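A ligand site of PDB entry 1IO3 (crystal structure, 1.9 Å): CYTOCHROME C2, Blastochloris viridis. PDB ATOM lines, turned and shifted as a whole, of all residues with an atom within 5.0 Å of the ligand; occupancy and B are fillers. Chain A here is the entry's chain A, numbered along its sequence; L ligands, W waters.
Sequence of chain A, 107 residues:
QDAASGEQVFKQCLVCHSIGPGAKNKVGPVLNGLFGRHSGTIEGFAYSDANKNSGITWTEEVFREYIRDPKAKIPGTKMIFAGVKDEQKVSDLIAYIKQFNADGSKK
The side-chain sulfur of Cys 16 is covalently linked to a carbon (C25) of the ligand, at 1.8 Å.
The side-chain sulfur (SG) of Cys 13 is bonded to a carbon (C18) of the ligand, 1.8 Å away.
An iron atom (FE1) of the ligand is bound by a ring nitrogen (NE2) of His 17, at 1.9 Å.
The side-chain sulfur of Met 79 binds an iron atom (FE1) of the ligand, at 2.1 Å.
The side-chain hydroxyl (OH) of Tyr 47 lies within hydrogen-bond range of an oxygen (O2) of the ligand, 2.5 Å away.
N of Ser 48 lies within hydrogen-bond range of O4 of the ligand, 3.0 Å away.
The side-chain hydroxyl (OG) of Ser 48 sits at hydrogen-bond distance from an oxygen (O3) of the ligand (2.8 Å).
An oxygen (O3) of the ligand lies within hydrogen-bond range of the side-chain hydroxyl of Thr 77 (2.8 Å).
O3 of the ligand lies within hydrogen-bond range of N of Lys 78 (2.9 Å).
O1 of the ligand lies within hydrogen-bond range of N of Gly 40 (3.0 Å).
NE1 of Trp 58 lies within hydrogen-bond range of O1 of the ligand, 3.1 Å away.
The side-chain amide oxygen (OD1) of Asn 51 lies close to an oxygen (O1) of the ligand, at 3.2 Å.
NH1 of Arg 37 is in salt-bridge range of O2 of the ligand (3.3 Å).
The backbone carbonyl oxygen (O) of Cys 16 is in hydrogen-bond range of the backbone NH (N) of Gly 28 (2.9 Å).
The backbone NH of Met 79 lies close to the side-chain hydroxyl of Thr 77 (3.4 Å).
The side-chain sulfur (SD) of Met 79 sits close to the side-chain hydroxyl (OH) of Tyr 66, at 3.2 Å.
OH of Tyr 47 is in hydrogen-bond range of N of Ile 42.
The side-chain amide oxygen (OD1) of Asn 51 lies within hydrogen-bond range of the backbone NH (N) of Gly 40, 3.3 Å away.
N of Trp 58 is in hydrogen-bond range of O of Arg 37 (3.0 Å).
OG of Ser 39 lies within hydrogen-bond range of O of Asn 51, at 3.3 Å.
O of Ile 67 lies within hydrogen-bond range of N of Val 84 (2.6 Å).
Merely in contact with the ligand: Gln 12 (3.3 Å), Val 27 (3.4 Å), Gly 28 (3.8 Å), Pro 29 (3.6 Å), Leu 31 (3.95 Å), Leu 34 (3.9 Å), Ser 39 (3.4 Å), Phe 45 (3.6 Å), Phe 63 (3.6 Å), Tyr 66 (3.5 Å), Ile 67 (3.6 Å), Phe 81 (3.6 Å), Val 84 (3.7 Å) and Leu 93 (3.98 Å).
Hydrophobic or aromatic side chains that line the ligand: His 17, Pro 29, Leu 31, Leu 34, Phe 45, Tyr 47, Trp 58, Phe 63, Tyr 66, Ile 67, Met 79, Phe 81, Val 84 and Leu 93.
26 residues have an atom within 4 Å of the ligand: Gln 12, Cys 13, Cys 16, His 17, Val 27, Gly 28, Pro 29, Leu 31, Leu 34, Arg 37, Ser 39, Gly 40, Phe 45, Tyr 47, Ser 48, Asn 51, Trp 58, Phe 63, Tyr 66, Ile 67, Thr 77, Lys 78, Met 79, Phe 81, Val 84 and Leu 93.
Along chain A the residues within 4 Å of the ligand span positions 12 to 93.
The nearest printed residue that does not touch the ligand is Ile 97 (4.1 Å).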
ATOM      1  N   GLN A  12       7.631  -8.040   7.032  1.00  0.00           N
ATOM      2  CA  GLN A  12       7.933  -8.908   8.175  1.00  0.00           C
ATOM      3  C   GLN A  12       6.629  -9.315   8.827  1.00  0.00           C
ATOM      4  O   GLN A  12       6.536 -10.383   9.430  1.00  0.00           O
ATOM      5  CB  GLN A  12       8.854  -8.226   9.206  1.00  0.00           C
ATOM      6  CG  GLN A  12       8.609  -6.766   9.483  1.00  0.00           C
ATOM      7  CD  GLN A  12       9.773  -6.127  10.230  1.00  0.00           C
ATOM      8  OE1 GLN A  12      10.135  -4.978   9.991  1.00  0.00           O
ATOM      9  NE2 GLN A  12      10.375  -6.885  11.150  1.00  0.00           N
ATOM     10  N   CYS A  13       5.607  -8.464   8.704  1.00  0.00           N
ATOM     11  CA  CYS A  13       4.289  -8.779   9.264  1.00  0.00           C
ATOM     12  C   CYS A  13       3.523  -9.759   8.382  1.00  0.00           C
ATOM     13  O   CYS A  13       2.786 -10.603   8.891  1.00  0.00           O
ATOM     14  CB  CYS A  13       3.432  -7.524   9.402  1.00  0.00           C
ATOM     15  SG  CYS A  13       4.260  -6.044  10.035  1.00  0.00           S
ATOM     16  N   CYS A  16       2.703 -13.569   9.041  1.00  0.00           N
ATOM     17  CA  CYS A  16       1.638 -13.998   9.952  1.00  0.00           C
ATOM     18  C   CYS A  16       0.336 -13.250   9.761  1.00  0.00           C
ATOM     19  O   CYS A  16      -0.728 -13.750  10.122  1.00  0.00           O
ATOM     20  CB  CYS A  16       2.073 -13.810  11.402  1.00  0.00           C
ATOM     21  SG  CYS A  16       3.663 -14.571  11.843  1.00  0.00           S
ATOM     22  N   HIS A  17       0.400 -12.059   9.179  1.00  0.00           N
ATOM     23  CA  HIS A  17      -0.771 -11.223   8.966  1.00  0.00           C
ATOM     24  C   HIS A  17      -1.088 -10.958   7.481  1.00  0.00           C
ATOM     25  O   HIS A  17      -0.195 -10.817   6.663  1.00  0.00           O
ATOM     26  CB  HIS A  17      -0.597  -9.864   9.651  1.00  0.00           C
ATOM     27  CG  HIS A  17      -0.505  -9.927  11.135  1.00  0.00           C
ATOM     28  ND1 HIS A  17      -1.588 -10.115  11.977  1.00  0.00           N
ATOM     29  CD2 HIS A  17       0.548  -9.694  11.965  1.00  0.00           C
ATOM     30  CE1 HIS A  17      -1.164  -9.990  13.230  1.00  0.00           C
ATOM     31  NE2 HIS A  17       0.132  -9.729  13.289  1.00  0.00           N
ATOM     32  N   VAL A  27      -1.654 -17.073  11.097  1.00  0.00           N
ATOM     33  CA  VAL A  27      -1.103 -17.253  12.441  1.00  0.00           C
ATOM     34  C   VAL A  27      -1.580 -16.044  13.264  1.00  0.00           C
ATOM     35  O   VAL A  27      -1.831 -16.163  14.458  1.00  0.00           O
ATOM     36  CB  VAL A  27       0.434 -17.312  12.408  1.00  0.00           C
ATOM     37  CG1 VAL A  27       1.006 -17.141  13.807  1.00  0.00           C
ATOM     38  CG2 VAL A  27       0.882 -18.655  11.835  1.00  0.00           C
ATOM     39  N   GLY A  28      -1.711 -14.905  12.598  1.00  0.00           N
ATOM     40  CA  GLY A  28      -2.164 -13.684  13.256  1.00  0.00           C
ATOM     41  C   GLY A  28      -3.456 -13.209  12.605  1.00  0.00           C
ATOM     42  O   GLY A  28      -3.799 -13.674  11.520  1.00  0.00           O
ATOM     43  N   PRO A  29      -4.188 -12.283  13.249  1.00  0.00           N
ATOM     44  CA  PRO A  29      -5.451 -11.762  12.709  1.00  0.00           C
ATOM     45  C   PRO A  29      -5.301 -10.785  11.545  1.00  0.00           C
ATOM     46  O   PRO A  29      -4.255 -10.161  11.378  1.00  0.00           O
ATOM     47  CB  PRO A  29      -6.135 -11.110  13.917  1.00  0.00           C
ATOM     48  CG  PRO A  29      -5.012 -10.752  14.837  1.00  0.00           C
ATOM     49  CD  PRO A  29      -3.861 -11.682  14.553  1.00  0.00           C
ATOM     50  N   LEU A  31      -5.399  -7.514   9.460  1.00  0.00           N
ATOM     51  CA  LEU A  31      -5.135  -6.155   9.900  1.00  0.00           C
ATOM     52  C   LEU A  31      -5.846  -5.065   9.096  1.00  0.00           C
ATOM     53  O   LEU A  31      -5.418  -3.908   9.115  1.00  0.00           O
ATOM     54  CB  LEU A  31      -3.616  -5.884   9.920  1.00  0.00           C
ATOM     55  CG  LEU A  31      -2.763  -6.708  10.890  1.00  0.00           C
ATOM     56  CD1 LEU A  31      -1.334  -6.228  10.831  1.00  0.00           C
ATOM     57  CD2 LEU A  31      -3.299  -6.598  12.312  1.00  0.00           C
ATOM     58  N   LEU A  34      -7.490  -1.602  11.023  1.00  0.00           N
ATOM     59  CA  LEU A  34      -6.931  -1.765  12.358  1.00  0.00           C
ATOM     60  C   LEU A  34      -7.156  -0.586  13.300  1.00  0.00           C
ATOM     61  O   LEU A  34      -7.636  -0.756  14.428  1.00  0.00           O
ATOM     62  CB  LEU A  34      -5.426  -2.033  12.272  1.00  0.00           C
ATOM     63  CG  LEU A  34      -4.641  -2.002  13.595  1.00  0.00           C
ATOM     64  CD1 LEU A  34      -5.159  -3.122  14.513  1.00  0.00           C
ATOM     65  CD2 LEU A  34      -3.165  -2.205  13.306  1.00  0.00           C
ATOM     66  N   ARG A  37     -10.061   0.271  16.039  1.00  0.00           N
ATOM     67  CA  ARG A  37     -10.689  -0.956  16.521  1.00  0.00           C
ATOM     68  C   ARG A  37     -10.165  -1.407  17.882  1.00  0.00           C
ATOM     69  O   ARG A  37      -9.017  -1.160  18.246  1.00  0.00           O
ATOM     70  CB  ARG A  37     -10.556  -2.044  15.440  1.00  0.00           C
ATOM     71  CG  ARG A  37      -9.764  -3.293  15.762  1.00  0.00           C
ATOM     72  CD  ARG A  37      -9.778  -4.213  14.548  1.00  0.00           C
ATOM     73  NE  ARG A  37      -8.750  -5.251  14.620  1.00  0.00           N
ATOM     74  CZ  ARG A  37      -7.994  -5.658  13.593  1.00  0.00           C
ATOM     75  NH1 ARG A  37      -7.113  -6.636  13.767  1.00  0.00           N
ATOM     76  NH2 ARG A  37      -8.142  -5.126  12.389  1.00  0.00           N
ATOM     77  N   HIS A  38     -11.040  -2.045  18.658  1.00  0.00           N
ATOM     78  CA  HIS A  38     -10.661  -2.523  19.981  1.00  0.00           C
ATOM     79  C   HIS A  38      -9.888  -3.834  19.846  1.00  0.00           C
ATOM     80  O   HIS A  38     -10.186  -4.657  18.980  1.00  0.00           O
ATOM     81  CB  HIS A  38     -11.910  -2.675  20.859  1.00  0.00           C
ATOM     82  CG  HIS A  38     -12.477  -1.360  21.297  1.00  0.00           C
ATOM     83  ND1 HIS A  38     -12.372  -0.893  22.592  1.00  0.00           N
ATOM     84  CD2 HIS A  38     -13.115  -0.382  20.597  1.00  0.00           C
ATOM     85  CE1 HIS A  38     -12.914   0.308  22.674  1.00  0.00           C
ATOM     86  NE2 HIS A  38     -13.372   0.647  21.481  1.00  0.00           N
ATOM     87  N   SER A  39      -8.874  -3.996  20.682  1.00  0.00           N
ATOM     88  CA  SER A  39      -8.025  -5.168  20.646  1.00  0.00           C
ATOM     89  C   SER A  39      -8.783  -6.459  20.895  1.00  0.00           C
ATOM     90  O   SER A  39      -9.732  -6.484  21.676  1.00  0.00           O
ATOM     91  CB  SER A  39      -6.921  -5.032  21.685  1.00  0.00           C
ATOM     92  OG  SER A  39      -7.451  -5.147  22.988  1.00  0.00           O
ATOM     93  N   GLY A  40      -8.354  -7.516  20.223  1.00  0.00           N
ATOM     94  CA  GLY A  40      -8.981  -8.808  20.397  1.00  0.00           C
ATOM     95  C   GLY A  40     -10.397  -8.961  19.884  1.00  0.00           C
ATOM     96  O   GLY A  40     -11.159  -9.762  20.430  1.00  0.00           O
ATOM     97  N   THR A  41     -10.766  -8.254  18.819  1.00  0.00           N
ATOM     98  CA  THR A  41     -12.129  -8.370  18.307  1.00  0.00           C
ATOM     99  C   THR A  41     -12.332  -8.838  16.855  1.00  0.00           C
ATOM    100  O   THR A  41     -13.465  -8.923  16.395  1.00  0.00           O
ATOM    101  CB  THR A  41     -12.911  -7.035  18.478  1.00  0.00           C
ATOM    102  OG1 THR A  41     -12.286  -6.005  17.714  1.00  0.00           O
ATOM    103  CG2 THR A  41     -12.953  -6.636  19.953  1.00  0.00           C
ATOM    104  N   ILE A  42     -11.259  -9.136  16.126  1.00  0.00           N
ATOM    105  CA  ILE A  42     -11.412  -9.610  14.753  1.00  0.00           C
ATOM    106  C   ILE A  42     -12.104 -10.975  14.826  1.00  0.00           C
ATOM    107  O   ILE A  42     -11.652 -11.860  15.537  1.00  0.00           O
ATOM    108  CB  ILE A  42     -10.053  -9.770  14.026  1.00  0.00           C
ATOM    109  CG1 ILE A  42      -9.611  -8.420  13.452  1.00  0.00           C
ATOM    110  CG2 ILE A  42     -10.161 -10.784  12.897  1.00  0.00           C
ATOM    111  CD1 ILE A  42     -10.649  -7.767  12.551  1.00  0.00           C
ATOM    112  N   PHE A  45     -10.733 -15.195  14.991  1.00  0.00           N
ATOM    113  CA  PHE A  45      -9.397 -15.407  15.509  1.00  0.00           C
ATOM    114  C   PHE A  45      -9.361 -15.785  16.971  1.00  0.00           C
ATOM    115  O   PHE A  45     -10.124 -15.251  17.771  1.00  0.00           O
ATOM    116  CB  PHE A  45      -8.525 -14.172  15.278  1.00  0.00           C
ATOM    117  CG  PHE A  45      -7.074 -14.410  15.569  1.00  0.00           C
ATOM    118  CD1 PHE A  45      -6.285 -15.148  14.686  1.00  0.00           C
ATOM    119  CD2 PHE A  45      -6.520 -13.964  16.756  1.00  0.00           C
ATOM    120  CE1 PHE A  45      -4.971 -15.437  14.990  1.00  0.00           C
ATOM    121  CE2 PHE A  45      -5.202 -14.239  17.069  1.00  0.00           C
ATOM    122  CZ  PHE A  45      -4.423 -14.985  16.183  1.00  0.00           C
ATOM    123  N   ALA A  46      -8.482 -16.721  17.314  1.00  0.00           N
ATOM    124  CA  ALA A  46      -8.346 -17.177  18.695  1.00  0.00           C
ATOM    125  C   ALA A  46      -7.239 -16.392  19.391  1.00  0.00           C
ATOM    126  O   ALA A  46      -6.073 -16.766  19.339  1.00  0.00           O
ATOM    127  CB  ALA A  46      -8.035 -18.670  18.737  1.00  0.00           C
ATOM    128  N   TYR A  47      -7.623 -15.304  20.045  1.00  0.00           N
ATOM    129  CA  TYR A  47      -6.688 -14.446  20.751  1.00  0.00           C
ATOM    130  C   TYR A  47      -6.300 -15.031  22.087  1.00  0.00           C
ATOM    131  O   TYR A  47      -7.001 -15.873  22.631  1.00  0.00           O
ATOM    132  CB  TYR A  47      -7.308 -13.081  21.028  1.00  0.00           C
ATOM    133  CG  TYR A  47      -7.470 -12.179  19.842  1.00  0.00           C
ATOM    134  CD1 TYR A  47      -8.694 -12.109  19.179  1.00  0.00           C
ATOM    135  CD2 TYR A  47      -6.437 -11.360  19.406  1.00  0.00           C
ATOM    136  CE1 TYR A  47      -8.876 -11.243  18.114  1.00  0.00           C
ATOM    137  CE2 TYR A  47      -6.616 -10.487  18.337  1.00  0.00           C
ATOM    138  CZ  TYR A  47      -7.840 -10.432  17.690  1.00  0.00           C
ATOM    139  OH  TYR A  47      -8.055  -9.566  16.644  1.00  0.00           O
ATOM    140  N   SER A  48      -5.167 -14.571  22.608  1.00  0.00           N
ATOM    141  CA  SER A  48      -4.716 -14.987  23.926  1.00  0.00           C
ATOM    142  C   SER A  48      -5.560 -14.135  24.885  1.00  0.00           C
ATOM    143  O   SER A  48      -6.174 -13.158  24.459  1.00  0.00           O
ATOM    144  CB  SER A  48      -3.225 -14.663  24.112  1.00  0.00           C
ATOM    145  OG  SER A  48      -3.014 -13.260  24.220  1.00  0.00           O
ATOM    146  N   ASN A  51      -4.166 -10.566  25.084  1.00  0.00           N
ATOM    147  CA  ASN A  51      -4.559  -9.653  24.015  1.00  0.00           C
ATOM    148  C   ASN A  51      -6.042  -9.290  24.115  1.00  0.00           C
ATOM    149  O   ASN A  51      -6.423  -8.124  24.066  1.00  0.00           O
ATOM    150  CB  ASN A  51      -4.301 -10.317  22.667  1.00  0.00           C
ATOM    151  CG  ASN A  51      -4.468  -9.367  21.497  1.00  0.00           C
ATOM    152  OD1 ASN A  51      -5.496  -8.704  21.363  1.00  0.00           O
ATOM    153  ND2 ASN A  51      -3.461  -9.318  20.627  1.00  0.00           N
ATOM    154  N   TRP A  58      -6.872   0.531  19.458  1.00  0.00           N
ATOM    155  CA  TRP A  58      -5.748   0.855  18.609  1.00  0.00           C
ATOM    156  C   TRP A  58      -5.769   2.223  17.988  1.00  0.00           C
ATOM    157  O   TRP A  58      -6.503   2.475  17.035  1.00  0.00           O
ATOM    158  CB  TRP A  58      -5.610  -0.203  17.521  1.00  0.00           C
ATOM    159  CG  TRP A  58      -5.260  -1.550  18.080  1.00  0.00           C
ATOM    160  CD1 TRP A  58      -6.043  -2.670  18.073  1.00  0.00           C
ATOM    161  CD2 TRP A  58      -4.015  -1.922  18.699  1.00  0.00           C
ATOM    162  NE1 TRP A  58      -5.360  -3.722  18.648  1.00  0.00           N
ATOM    163  CE2 TRP A  58      -4.119  -3.298  19.035  1.00  0.00           C
ATOM    164  CE3 TRP A  58      -2.832  -1.247  19.000  1.00  0.00           C
ATOM    165  CZ2 TRP A  58      -3.074  -3.995  19.650  1.00  0.00           C
ATOM    166  CZ3 TRP A  58      -1.787  -1.944  19.615  1.00  0.00           C
ATOM    167  CH2 TRP A  58      -1.932  -3.311  19.934  1.00  0.00           C
ATOM    168  N   PHE A  63      -0.403   2.157  19.009  1.00  0.00           N
ATOM    169  CA  PHE A  63       0.196   1.200  18.075  1.00  0.00           C
ATOM    170  C   PHE A  63       1.716   1.356  18.017  1.00  0.00           C
ATOM    171  O   PHE A  63       2.454   0.378  17.951  1.00  0.00           O
ATOM    172  CB  PHE A  63      -0.397   1.357  16.676  1.00  0.00           C
ATOM    173  CG  PHE A  63       0.305   0.542  15.616  1.00  0.00           C
ATOM    174  CD1 PHE A  63      -0.061  -0.787  15.375  1.00  0.00           C
ATOM    175  CD2 PHE A  63       1.334   1.095  14.861  1.00  0.00           C
ATOM    176  CE1 PHE A  63       0.604  -1.556  14.391  1.00  0.00           C
ATOM    177  CE2 PHE A  63       2.001   0.347  13.874  1.00  0.00           C
ATOM    178  CZ  PHE A  63       1.629  -0.976  13.639  1.00  0.00           C
ATOM    179  N   TYR A  66       3.361  -0.126  21.114  1.00  0.00           N
ATOM    180  CA  TYR A  66       3.244  -1.590  21.044  1.00  0.00           C
ATOM    181  C   TYR A  66       4.224  -2.266  20.050  1.00  0.00           C
ATOM    182  O   TYR A  66       4.939  -3.201  20.415  1.00  0.00           O
ATOM    183  CB  TYR A  66       1.807  -1.961  20.678  1.00  0.00           C
ATOM    184  CG  TYR A  66       1.612  -3.396  20.246  1.00  0.00           C
ATOM    185  CD1 TYR A  66       1.557  -3.735  18.892  1.00  0.00           C
ATOM    186  CD2 TYR A  66       1.424  -4.416  21.181  1.00  0.00           C
ATOM    187  CE1 TYR A  66       1.339  -5.047  18.488  1.00  0.00           C
ATOM    188  CE2 TYR A  66       1.202  -5.736  20.781  1.00  0.00           C
ATOM    189  CZ  TYR A  66       1.154  -6.038  19.433  1.00  0.00           C
ATOM    190  OH  TYR A  66       0.928  -7.331  19.035  1.00  0.00           O
ATOM    191  N   ILE A  67       4.246  -1.798  18.808  1.00  0.00           N
ATOM    192  CA  ILE A  67       5.101  -2.391  17.792  1.00  0.00           C
ATOM    193  C   ILE A  67       6.588  -2.283  18.123  1.00  0.00           C
ATOM    194  O   ILE A  67       7.396  -3.059  17.621  1.00  0.00           O
ATOM    195  CB  ILE A  67       4.827  -1.769  16.397  1.00  0.00           C
ATOM    196  CG1 ILE A  67       5.015  -2.834  15.315  1.00  0.00           C
ATOM    197  CG2 ILE A  67       5.724  -0.571  16.142  1.00  0.00           C
ATOM    198  CD1 ILE A  67       4.086  -4.000  15.486  1.00  0.00           C
ATOM    199  N   THR A  77       1.479 -12.111  25.384  1.00  0.00           N
ATOM    200  CA  THR A  77       0.904 -12.179  24.037  1.00  0.00           C
ATOM    201  C   THR A  77       1.549 -13.297  23.210  1.00  0.00           C
ATOM    202  O   THR A  77       2.720 -13.627  23.405  1.00  0.00           O
ATOM    203  CB  THR A  77       1.075 -10.848  23.283  1.00  0.00           C
ATOM    204  OG1 THR A  77       0.359 -10.913  22.050  1.00  0.00           O
ATOM    205  CG2 THR A  77       2.544 -10.563  22.984  1.00  0.00           C
ATOM    206  N   LYS A  78       0.764 -13.860  22.291  1.00  0.00           N
ATOM    207  CA  LYS A  78       1.225 -14.937  21.404  1.00  0.00           C
ATOM    208  C   LYS A  78       2.071 -14.418  20.239  1.00  0.00           C
ATOM    209  O   LYS A  78       2.692 -15.190  19.513  1.00  0.00           O
ATOM    210  CB  LYS A  78       0.041 -15.693  20.811  1.00  0.00           C
ATOM    211  CG  LYS A  78      -0.746 -16.557  21.769  1.00  0.00           C
ATOM    212  CD  LYS A  78      -2.096 -16.868  21.130  1.00  0.00           C
ATOM    213  CE  LYS A  78      -2.743 -18.108  21.731  1.00  0.00           C
ATOM    214  NZ  LYS A  78      -3.847 -18.581  20.842  1.00  0.00           N
ATOM    215  N   MET A  79       2.061 -13.095  20.050  1.00  0.00           N
ATOM    216  CA  MET A  79       2.822 -12.482  18.964  1.00  0.00           C
ATOM    217  C   MET A  79       4.276 -12.388  19.400  1.00  0.00           C
ATOM    218  O   MET A  79       4.730 -11.321  19.825  1.00  0.00           O
ATOM    219  CB  MET A  79       2.277 -11.073  18.652  1.00  0.00           C
ATOM    220  CG  MET A  79       3.108 -10.290  17.628  1.00  0.00           C
ATOM    221  SD  MET A  79       2.206  -9.020  16.649  1.00  0.00           S
ATOM    222  CE  MET A  79       3.444  -7.716  16.684  1.00  0.00           C
ATOM    223  N   ILE A  80       5.000 -13.503  19.316  1.00  0.00           N
ATOM    224  CA  ILE A  80       6.394 -13.499  19.691  1.00  0.00           C
ATOM    225  C   ILE A  80       7.078 -12.929  18.459  1.00  0.00           C
ATOM    226  O   ILE A  80       7.323 -13.619  17.465  1.00  0.00           O
ATOM    227  CB  ILE A  80       6.905 -14.904  20.051  1.00  0.00           C
ATOM    228  CG1 ILE A  80       6.147 -15.408  21.296  1.00  0.00           C
ATOM    229  CG2 ILE A  80       8.380 -14.851  20.426  1.00  0.00           C
ATOM    230  CD1 ILE A  80       6.171 -16.923  21.484  1.00  0.00           C
ATOM    231  N   PHE A  81       7.333 -11.632  18.544  1.00  0.00           N
ATOM    232  CA  PHE A  81       7.924 -10.846  17.475  1.00  0.00           C
ATOM    233  C   PHE A  81       8.731  -9.798  18.242  1.00  0.00           C
ATOM    234  O   PHE A  81       8.244  -9.267  19.232  1.00  0.00           O
ATOM    235  CB  PHE A  81       6.797 -10.222  16.650  1.00  0.00           C
ATOM    236  CG  PHE A  81       7.241  -9.140  15.710  1.00  0.00           C
ATOM    237  CD1 PHE A  81       7.975  -9.461  14.572  1.00  0.00           C
ATOM    238  CD2 PHE A  81       6.931  -7.810  15.962  1.00  0.00           C
ATOM    239  CE1 PHE A  81       8.404  -8.473  13.695  1.00  0.00           C
ATOM    240  CE2 PHE A  81       7.354  -6.817  15.091  1.00  0.00           C
ATOM    241  CZ  PHE A  81       8.097  -7.151  13.958  1.00  0.00           C
ATOM    242  N   VAL A  84       9.438  -3.328  16.019  1.00  0.00           N
ATOM    243  CA  VAL A  84      10.104  -2.434  15.081  1.00  0.00           C
ATOM    244  C   VAL A  84      10.600  -1.221  15.865  1.00  0.00           C
ATOM    245  O   VAL A  84       9.803  -0.410  16.326  1.00  0.00           O
ATOM    246  CB  VAL A  84       9.129  -1.989  13.960  1.00  0.00           C
ATOM    247  CG1 VAL A  84       9.881  -1.180  12.914  1.00  0.00           C
ATOM    248  CG2 VAL A  84       8.466  -3.198  13.315  1.00  0.00           C
ATOM    249  N   LEU A  93       5.103   2.362   8.257  1.00  0.00           N
ATOM    250  CA  LEU A  93       4.265   1.195   8.507  1.00  0.00           C
ATOM    251  C   LEU A  93       2.836   1.691   8.743  1.00  0.00           C
ATOM    252  O   LEU A  93       1.890   1.190   8.123  1.00  0.00           O
ATOM    253  CB  LEU A  93       4.807   0.429   9.728  1.00  0.00           C
ATOM    254  CG  LEU A  93       4.140  -0.877  10.142  1.00  0.00           C
ATOM    255  CD1 LEU A  93       4.093  -1.848   8.963  1.00  0.00           C
ATOM    256  CD2 LEU A  93       4.905  -1.467  11.313  1.00  0.00           C
ATOM    257  N   ILE A  97      -0.656   0.709   6.581  1.00  0.00           N
ATOM    258  CA  ILE A  97      -1.823   0.051   7.155  1.00  0.00           C
ATOM    259  C   ILE A  97      -3.074   0.939   7.088  1.00  0.00           C
ATOM    260  O   ILE A  97      -4.164   0.448   6.823  1.00  0.00           O
ATOM    261  CB  ILE A  97      -1.567  -0.388   8.627  1.00  0.00           C
ATOM    262  CG1 ILE A  97      -0.508  -1.491   8.674  1.00  0.00           C
ATOM    263  CG2 ILE A  97      -2.871  -0.935   9.245  1.00  0.00           C
ATOM    264  CD1 ILE A  97       0.079  -1.740  10.056  1.00  0.00           C
HETATM  265 FE1  LIG L   1       1.150  -9.386  14.826  1.00  0.00          FE
HETATM  266  C1  LIG L   1      -1.502  -9.658  16.904  1.00  0.00           C
HETATM  267  C2  LIG L   1       0.471  -6.121  14.343  1.00  0.00           C
HETATM  268  C3  LIG L   1       4.046  -9.037  13.038  1.00  0.00           C
HETATM  269  C4  LIG L   1       1.607 -12.747  14.957  1.00  0.00           C
HETATM  270  N1  LIG L   1      -0.114  -8.118  15.625  1.00  0.00           N
HETATM  271  C5  LIG L   1      -1.159  -8.380  16.476  1.00  0.00           C
HETATM  272  C6  LIG L   1      -1.931  -7.171  16.788  1.00  0.00           C
HETATM  273  C7  LIG L   1      -1.339  -6.173  16.073  1.00  0.00           C
HETATM  274  C8  LIG L   1      -0.274  -6.790  15.288  1.00  0.00           C
HETATM  275  C9  LIG L   1      -1.750  -4.702  16.019  1.00  0.00           C
HETATM  276  C10 LIG L   1      -3.197  -7.024  17.663  1.00  0.00           C
HETATM  277  C11 LIG L   1      -4.420  -7.428  16.845  1.00  0.00           C
HETATM  278  C12 LIG L   1      -5.754  -7.213  17.558  1.00  0.00           C
HETATM  279  O1  LIG L   1      -5.769  -6.842  18.752  1.00  0.00           O
HETATM  280  O2  LIG L   1      -6.790  -7.431  16.909  1.00  0.00           O
HETATM  281  N2  LIG L   1       2.065  -7.884  13.868  1.00  0.00           N
HETATM  282  C13 LIG L   1       1.573  -6.609  13.696  1.00  0.00           C
HETATM  283  C14 LIG L   1       2.438  -5.802  12.862  1.00  0.00           C
HETATM  284  C15 LIG L   1       3.510  -6.612  12.551  1.00  0.00           C
HETATM  285  C16 LIG L   1       3.263  -7.900  13.180  1.00  0.00           C
HETATM  286  C17 LIG L   1       2.178  -4.366  12.434  1.00  0.00           C
HETATM  287  C18 LIG L   1       4.767  -6.416  11.690  1.00  0.00           C
HETATM  288  C19 LIG L   1       5.582  -5.270  12.258  1.00  0.00           C
HETATM  289  N3  LIG L   1       2.570 -10.638  14.124  1.00  0.00           N
HETATM  290  C20 LIG L   1       3.738 -10.314  13.430  1.00  0.00           C
HETATM  291  C21 LIG L   1       4.509 -11.487  13.117  1.00  0.00           C
HETATM  292  C22 LIG L   1       3.769 -12.537  13.601  1.00  0.00           C
HETATM  293  C23 LIG L   1       2.567 -12.009  14.260  1.00  0.00           C
HETATM  294  C24 LIG L   1       5.885 -11.555  12.439  1.00  0.00           C
HETATM  295  C25 LIG L   1       3.914 -14.059  13.513  1.00  0.00           C
HETATM  296  C26 LIG L   1       5.302 -14.623  13.804  1.00  0.00           C
HETATM  297  N4  LIG L   1       0.167 -10.926  15.698  1.00  0.00           N
HETATM  298  C27 LIG L   1       0.524 -12.269  15.670  1.00  0.00           C
HETATM  299  C28 LIG L   1      -0.329 -13.045  16.575  1.00  0.00           C
HETATM  300  C29 LIG L   1      -1.288 -12.175  17.053  1.00  0.00           C
HETATM  301  C30 LIG L   1      -0.918 -10.850  16.553  1.00  0.00           C
HETATM  302  C31 LIG L   1      -0.212 -14.501  16.978  1.00  0.00           C
HETATM  303  C32 LIG L   1      -2.288 -12.508  18.132  1.00  0.00           C
HETATM  304  C33 LIG L   1      -1.546 -12.339  19.446  1.00  0.00           C
HETATM  305  C34 LIG L   1      -2.351 -12.782  20.650  1.00  0.00           C
HETATM  306  O3  LIG L   1      -1.843 -12.670  21.791  1.00  0.00           O
HETATM  307  O4  LIG L   1      -3.495 -13.238  20.451  1.00  0.00           O
HETATM  308  O   HOH W   1      -9.339  -6.395  17.183  1.00  0.00           O
